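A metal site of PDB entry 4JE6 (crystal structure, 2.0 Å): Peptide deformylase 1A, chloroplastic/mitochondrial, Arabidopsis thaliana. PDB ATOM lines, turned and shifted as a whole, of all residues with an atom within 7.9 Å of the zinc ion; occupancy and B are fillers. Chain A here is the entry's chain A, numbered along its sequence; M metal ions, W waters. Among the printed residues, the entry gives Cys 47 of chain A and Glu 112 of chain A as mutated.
ND1 of His 153 sits at hydrogen-bond distance from OE2 of Glu 109 (2.8 Å). The side-chain sulfur of Cys 111 lies close to the side-chain amide nitrogen of Gln 54 (3.4 Å). SG of Cys 111 sits close to N of Ser 113 (3.5 Å). The side-chain carboxylate (OE1) of Glu 154 sits close to the side-chain amide oxygen (OE1) of Gln 54 (3.4 Å). NE2 of Gln 54 sits at hydrogen-bond distance from OG of Ser 113 (3.1 Å). The side-chain amide oxygen (OE1) of Gln 54 is in hydrogen-bond range of the backbone NH (N) of Ala 51, at 3.0 Å. The backbone NH (N) of Leu 50 sits close to the side-chain carboxylate (OE1) of Glu 154 (3.5 Å). The side-chain carboxylate of Glu 154 lies within hydrogen-bond range of the backbone NH of Ala 51 (3.1 Å).
Merely in contact with the zinc ion: Gln 54 (3.6 Å) and Glu 154 (3.9 Å). The nearest printed residue that does not touch the zinc ion is Glu 112 (4.7 Å).
The zinc ion is bound by water W1, NE2 of His 157, NE2 of His 153 and SG of Cys 111.
Water W1 lies within hydrogen-bond range of OE2 of Glu 154 (2.5 Å) and OE1 of Gln 54 (2.8 Å).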
ATOM      1  N   LEU A  14       6.650 -25.084  24.440  1.00  0.00           N
ATOM      2  CA  LEU A  14       8.101 -24.977  24.620  1.00  0.00           C
ATOM      3  C   LEU A  14       8.537 -23.606  25.065  1.00  0.00           C
ATOM      4  O   LEU A  14       9.654 -23.427  25.540  1.00  0.00           O
ATOM      5  CB  LEU A  14       8.800 -25.247  23.273  1.00  0.00           C
ATOM      6  CG  LEU A  14       9.433 -26.592  22.933  1.00  0.00           C
ATOM      7  CD1 LEU A  14       9.044 -27.798  23.760  1.00  0.00           C
ATOM      8  CD2 LEU A  14       9.391 -26.881  21.454  1.00  0.00           C
ATOM      9  N   CYS A  47      19.458 -38.895  23.700  1.00  0.00           N
ATOM     10  CA  CYS A  47      20.027 -37.646  24.182  1.00  0.00           C
ATOM     11  C   CYS A  47      20.264 -37.737  25.696  1.00  0.00           C
ATOM     12  O   CYS A  47      19.899 -38.741  26.304  1.00  0.00           O
ATOM     13  CB  CYS A  47      19.149 -36.442  23.808  1.00  0.00           C
ATOM     14  SG  CYS A  47      17.501 -36.485  24.447  1.00  0.00           S
ATOM     15  N   GLY A  49      19.293 -35.340  28.093  1.00  0.00           N
ATOM     16  CA  GLY A  49      18.318 -34.699  28.953  1.00  0.00           C
ATOM     17  C   GLY A  49      17.018 -34.428  28.213  1.00  0.00           C
ATOM     18  O   GLY A  49      17.002 -34.306  26.989  1.00  0.00           O
ATOM     19  N   LEU A  50      15.934 -34.316  28.964  1.00  0.00           N
ATOM     20  CA  LEU A  50      14.630 -34.006  28.417  1.00  0.00           C
ATOM     21  C   LEU A  50      13.784 -33.323  29.475  1.00  0.00           C
ATOM     22  O   LEU A  50      13.896 -33.648  30.674  1.00  0.00           O
ATOM     23  CB  LEU A  50      13.938 -35.289  27.935  1.00  0.00           C
ATOM     24  CG  LEU A  50      12.896 -35.038  26.835  1.00  0.00           C
ATOM     25  CD1 LEU A  50      13.586 -34.861  25.460  1.00  0.00           C
ATOM     26  CD2 LEU A  50      11.895 -36.187  26.808  1.00  0.00           C
ATOM     27  N   ALA A  51      12.947 -32.372  29.034  1.00  0.00           N
ATOM     28  CA  ALA A  51      12.024 -31.672  29.940  1.00  0.00           C
ATOM     29  C   ALA A  51      10.587 -31.965  29.486  1.00  0.00           C
ATOM     30  O   ALA A  51      10.339 -32.184  28.281  1.00  0.00           O
ATOM     31  CB  ALA A  51      12.297 -30.163  29.915  1.00  0.00           C
ATOM     32  N   GLN A  54       8.845 -30.722  26.268  1.00  0.00           N
ATOM     33  CA  GLN A  54       9.316 -31.372  25.053  1.00  0.00           C
ATOM     34  C   GLN A  54       8.461 -32.583  24.640  1.00  0.00           C
ATOM     35  O   GLN A  54       8.559 -32.996  23.510  1.00  0.00           O
ATOM     36  CB  GLN A  54      10.790 -31.761  25.131  1.00  0.00           C
ATOM     37  CG  GLN A  54      11.749 -30.565  25.230  1.00  0.00           C
ATOM     38  CD  GLN A  54      13.167 -31.044  25.252  1.00  0.00           C
ATOM     39  OE1 GLN A  54      13.681 -31.431  26.288  1.00  0.00           O
ATOM     40  NE2 GLN A  54      13.787 -31.088  24.071  1.00  0.00           N
ATOM     41  N   GLU A 109      26.026 -26.764  22.526  1.00  0.00           N
ATOM     42  CA  GLU A 109      24.816 -27.508  22.903  1.00  0.00           C
ATOM     43  C   GLU A 109      23.897 -27.764  21.710  1.00  0.00           C
ATOM     44  O   GLU A 109      23.923 -27.003  20.751  1.00  0.00           O
ATOM     45  CB  GLU A 109      24.001 -26.698  23.926  1.00  0.00           C
ATOM     46  CG  GLU A 109      24.656 -26.601  25.285  1.00  0.00           C
ATOM     47  CD  GLU A 109      23.794 -25.890  26.315  1.00  0.00           C
ATOM     48  OE1 GLU A 109      24.398 -25.412  27.298  1.00  0.00           O
ATOM     49  OE2 GLU A 109      22.546 -25.791  26.149  1.00  0.00           O
ATOM     50  N   GLY A 110      23.079 -28.802  21.809  1.00  0.00           N
ATOM     51  CA  GLY A 110      21.984 -29.089  20.861  1.00  0.00           C
ATOM     52  C   GLY A 110      20.727 -29.295  21.687  1.00  0.00           C
ATOM     53  O   GLY A 110      20.795 -29.312  22.926  1.00  0.00           O
ATOM     54  N   CYS A 111      19.583 -29.424  21.022  1.00  0.00           N
ATOM     55  CA  CYS A 111      18.314 -29.691  21.700  1.00  0.00           C
ATOM     56  C   CYS A 111      17.487 -30.492  20.726  1.00  0.00           C
ATOM     57  O   CYS A 111      17.427 -30.148  19.559  1.00  0.00           O
ATOM     58  CB  CYS A 111      17.568 -28.412  22.073  1.00  0.00           C
ATOM     59  SG  CYS A 111      15.948 -28.719  22.935  1.00  0.00           S
ATOM     60  N   GLU A 112      16.836 -31.568  21.187  1.00  0.00           N
ATOM     61  CA  GLU A 112      16.054 -32.373  20.268  1.00  0.00           C
ATOM     62  C   GLU A 112      14.894 -31.581  19.660  1.00  0.00           C
ATOM     63  O   GLU A 112      14.362 -31.941  18.614  1.00  0.00           O
ATOM     64  CB  GLU A 112      15.526 -33.640  20.937  1.00  0.00           C
ATOM     65  CG  GLU A 112      16.601 -34.736  21.217  1.00  0.00           C
ATOM     66  CD  GLU A 112      17.382 -35.161  19.976  1.00  0.00           C
ATOM     67  OE1 GLU A 112      16.782 -35.478  18.927  1.00  0.00           O
ATOM     68  OE2 GLU A 112      18.614 -35.188  20.055  1.00  0.00           O
ATOM     69  N   SER A 113      14.496 -30.501  20.339  1.00  0.00           N
ATOM     70  CA  SER A 113      13.428 -29.618  19.851  1.00  0.00           C
ATOM     71  C   SER A 113      13.914 -28.619  18.765  1.00  0.00           C
ATOM     72  O   SER A 113      13.105 -27.886  18.181  1.00  0.00           O
ATOM     73  CB  SER A 113      12.762 -28.877  21.024  1.00  0.00           C
ATOM     74  OG  SER A 113      12.097 -29.817  21.862  1.00  0.00           O
ATOM     75  N   VAL A 114      15.221 -28.598  18.517  1.00  0.00           N
ATOM     76  CA  VAL A 114      15.808 -27.838  17.387  1.00  0.00           C
ATOM     77  C   VAL A 114      16.685 -28.822  16.622  1.00  0.00           C
ATOM     78  O   VAL A 114      17.896 -28.909  16.841  1.00  0.00           O
ATOM     79  CB  VAL A 114      16.667 -26.623  17.853  1.00  0.00           C
ATOM     80  CG1 VAL A 114      17.294 -25.861  16.637  1.00  0.00           C
ATOM     81  CG2 VAL A 114      15.863 -25.664  18.760  1.00  0.00           C
ATOM     82  N   ARG A 123      27.486 -21.419  30.423  1.00  0.00           N
ATOM     83  CA  ARG A 123      26.747 -22.008  31.550  1.00  0.00           C
ATOM     84  C   ARG A 123      27.556 -21.831  32.817  1.00  0.00           C
ATOM     85  O   ARG A 123      28.777 -21.665  32.731  1.00  0.00           O
ATOM     86  CB  ARG A 123      26.507 -23.524  31.323  1.00  0.00           C
ATOM     87  CG  ARG A 123      25.582 -23.910  30.139  1.00  0.00           C
ATOM     88  CD  ARG A 123      24.157 -23.382  30.283  1.00  0.00           C
ATOM     89  NE  ARG A 123      23.311 -23.847  29.177  1.00  0.00           N
ATOM     90  CZ  ARG A 123      22.006 -23.588  29.040  1.00  0.00           C
ATOM     91  NH1 ARG A 123      21.368 -22.841  29.920  1.00  0.00           N
ATOM     92  NH2 ARG A 123      21.336 -24.068  27.996  1.00  0.00           N
ATOM     93  N   ILE A 150      23.700 -29.755  31.612  1.00  0.00           N
ATOM     94  CA  ILE A 150      22.472 -30.450  31.235  1.00  0.00           C
ATOM     95  C   ILE A 150      21.333 -30.005  32.157  1.00  0.00           C
ATOM     96  O   ILE A 150      20.243 -29.673  31.702  1.00  0.00           O
ATOM     97  CB  ILE A 150      22.634 -31.977  31.281  1.00  0.00           C
ATOM     98  CG1 ILE A 150      23.710 -32.428  30.281  1.00  0.00           C
ATOM     99  CG2 ILE A 150      21.262 -32.699  31.014  1.00  0.00           C
ATOM    100  CD1 ILE A 150      24.143 -33.886  30.475  1.00  0.00           C
ATOM    101  N   HIS A 153      20.214 -26.472  31.078  1.00  0.00           N
ATOM    102  CA  HIS A 153      19.486 -26.563  29.810  1.00  0.00           C
ATOM    103  C   HIS A 153      18.044 -27.069  30.079  1.00  0.00           C
ATOM    104  O   HIS A 153      17.083 -26.484  29.586  1.00  0.00           O
ATOM    105  CB  HIS A 153      20.239 -27.522  28.885  1.00  0.00           C
ATOM    106  CG  HIS A 153      19.586 -27.731  27.556  1.00  0.00           C
ATOM    107  ND1 HIS A 153      20.176 -27.333  26.370  1.00  0.00           N
ATOM    108  CD2 HIS A 153      18.408 -28.319  27.211  1.00  0.00           C
ATOM    109  CE1 HIS A 153      19.384 -27.663  25.350  1.00  0.00           C
ATOM    110  NE2 HIS A 153      18.312 -28.274  25.842  1.00  0.00           N
ATOM    111  N   GLU A 154      17.922 -28.153  30.840  1.00  0.00           N
ATOM    112  CA  GLU A 154      16.600 -28.782  31.072  1.00  0.00           C
ATOM    113  C   GLU A 154      15.687 -27.938  31.965  1.00  0.00           C
ATOM    114  O   GLU A 154      14.487 -27.798  31.703  1.00  0.00           O
ATOM    115  CB  GLU A 154      16.743 -30.231  31.558  1.00  0.00           C
ATOM    116  CG  GLU A 154      17.457 -31.137  30.542  1.00  0.00           C
ATOM    117  CD  GLU A 154      16.823 -31.099  29.145  1.00  0.00           C
ATOM    118  OE1 GLU A 154      15.614 -30.861  29.037  1.00  0.00           O
ATOM    119  OE2 GLU A 154      17.542 -31.330  28.140  1.00  0.00           O
ATOM    120  N   ASP A 156      15.937 -24.642  32.179  1.00  0.00           N
ATOM    121  CA  ASP A 156      15.527 -23.568  31.253  1.00  0.00           C
ATOM    122  C   ASP A 156      14.240 -23.901  30.510  1.00  0.00           C
ATOM    123  O   ASP A 156      13.377 -23.029  30.374  1.00  0.00           O
ATOM    124  CB  ASP A 156      16.614 -23.267  30.213  1.00  0.00           C
ATOM    125  CG  ASP A 156      17.706 -22.351  30.745  1.00  0.00           C
ATOM    126  OD1 ASP A 156      18.662 -22.063  29.975  1.00  0.00           O
ATOM    127  OD2 ASP A 156      17.655 -21.924  31.912  1.00  0.00           O
ATOM    128  N   HIS A 157      14.101 -25.132  30.009  1.00  0.00           N
ATOM    129  CA  HIS A 157      12.860 -25.509  29.277  1.00  0.00           C
ATOM    130  C   HIS A 157      11.576 -25.241  30.077  1.00  0.00           C
ATOM    131  O   HIS A 157      10.520 -24.930  29.500  1.00  0.00           O
ATOM    132  CB  HIS A 157      12.855 -26.979  28.916  1.00  0.00           C
ATOM    133  CG  HIS A 157      13.616 -27.306  27.664  1.00  0.00           C
ATOM    134  ND1 HIS A 157      13.254 -26.843  26.423  1.00  0.00           N
ATOM    135  CD2 HIS A 157      14.708 -28.096  27.470  1.00  0.00           C
ATOM    136  CE1 HIS A 157      14.091 -27.304  25.516  1.00  0.00           C
ATOM    137  NE2 HIS A 157      14.981 -28.079  26.116  1.00  0.00           N
ATOM    138  N   ASN A 161      12.296 -21.396  28.066  1.00  0.00           N
ATOM    139  CA  ASN A 161      13.536 -20.865  27.472  1.00  0.00           C
ATOM    140  C   ASN A 161      14.385 -21.899  26.722  1.00  0.00           C
ATOM    141  O   ASN A 161      14.680 -22.960  27.289  1.00  0.00           O
ATOM    142  CB  ASN A 161      14.378 -20.177  28.549  1.00  0.00           C
ATOM    143  CG  ASN A 161      13.647 -19.050  29.228  1.00  0.00           C
ATOM    144  OD1 ASN A 161      12.943 -18.266  28.576  1.00  0.00           O
ATOM    145  ND2 ASN A 161      13.787 -18.959  30.550  1.00  0.00           N
ATOM    146  N   LEU A 162      14.744 -21.604  25.463  1.00  0.00           N
ATOM    147  CA  LEU A 162      15.606 -22.458  24.638  1.00  0.00           C
ATOM    148  C   LEU A 162      16.994 -21.851  24.469  1.00  0.00           C
ATOM    149  O   LEU A 162      17.159 -20.635  24.520  1.00  0.00           O
ATOM    150  CB  LEU A 162      14.989 -22.698  23.243  1.00  0.00           C
ATOM    151  CG  LEU A 162      13.569 -23.251  23.052  1.00  0.00           C
ATOM    152  CD1 LEU A 162      13.296 -23.738  21.632  1.00  0.00           C
ATOM    153  CD2 LEU A 162      13.225 -24.363  24.034  1.00  0.00           C
ATOM    154  N   TYR A 163      17.992 -22.709  24.215  1.00  0.00           N
ATOM    155  CA  TYR A 163      19.374 -22.236  24.098  1.00  0.00           C
ATOM    156  C   TYR A 163      19.589 -21.175  23.005  1.00  0.00           C
ATOM    157  O   TYR A 163      20.513 -20.341  23.104  1.00  0.00           O
ATOM    158  CB  TYR A 163      20.329 -23.422  23.924  1.00  0.00           C
ATOM    159  CG  TYR A 163      20.410 -23.978  22.523  1.00  0.00           C
ATOM    160  CD1 TYR A 163      21.353 -23.497  21.617  1.00  0.00           C
ATOM    161  CD2 TYR A 163      19.548 -25.001  22.114  1.00  0.00           C
ATOM    162  CE1 TYR A 163      21.439 -24.013  20.326  1.00  0.00           C
ATOM    163  CE2 TYR A 163      19.630 -25.525  20.813  1.00  0.00           C
ATOM    164  CZ  TYR A 163      20.583 -25.031  19.941  1.00  0.00           C
ATOM    165  OH  TYR A 163      20.688 -25.538  18.674  1.00  0.00           O
HETATM  166 ZN    ZN M   1      16.524 -29.079  25.143  1.00  0.00          ZN
HETATM  167  O   HOH W   1      16.381 -30.933  25.983  1.00  0.00           O
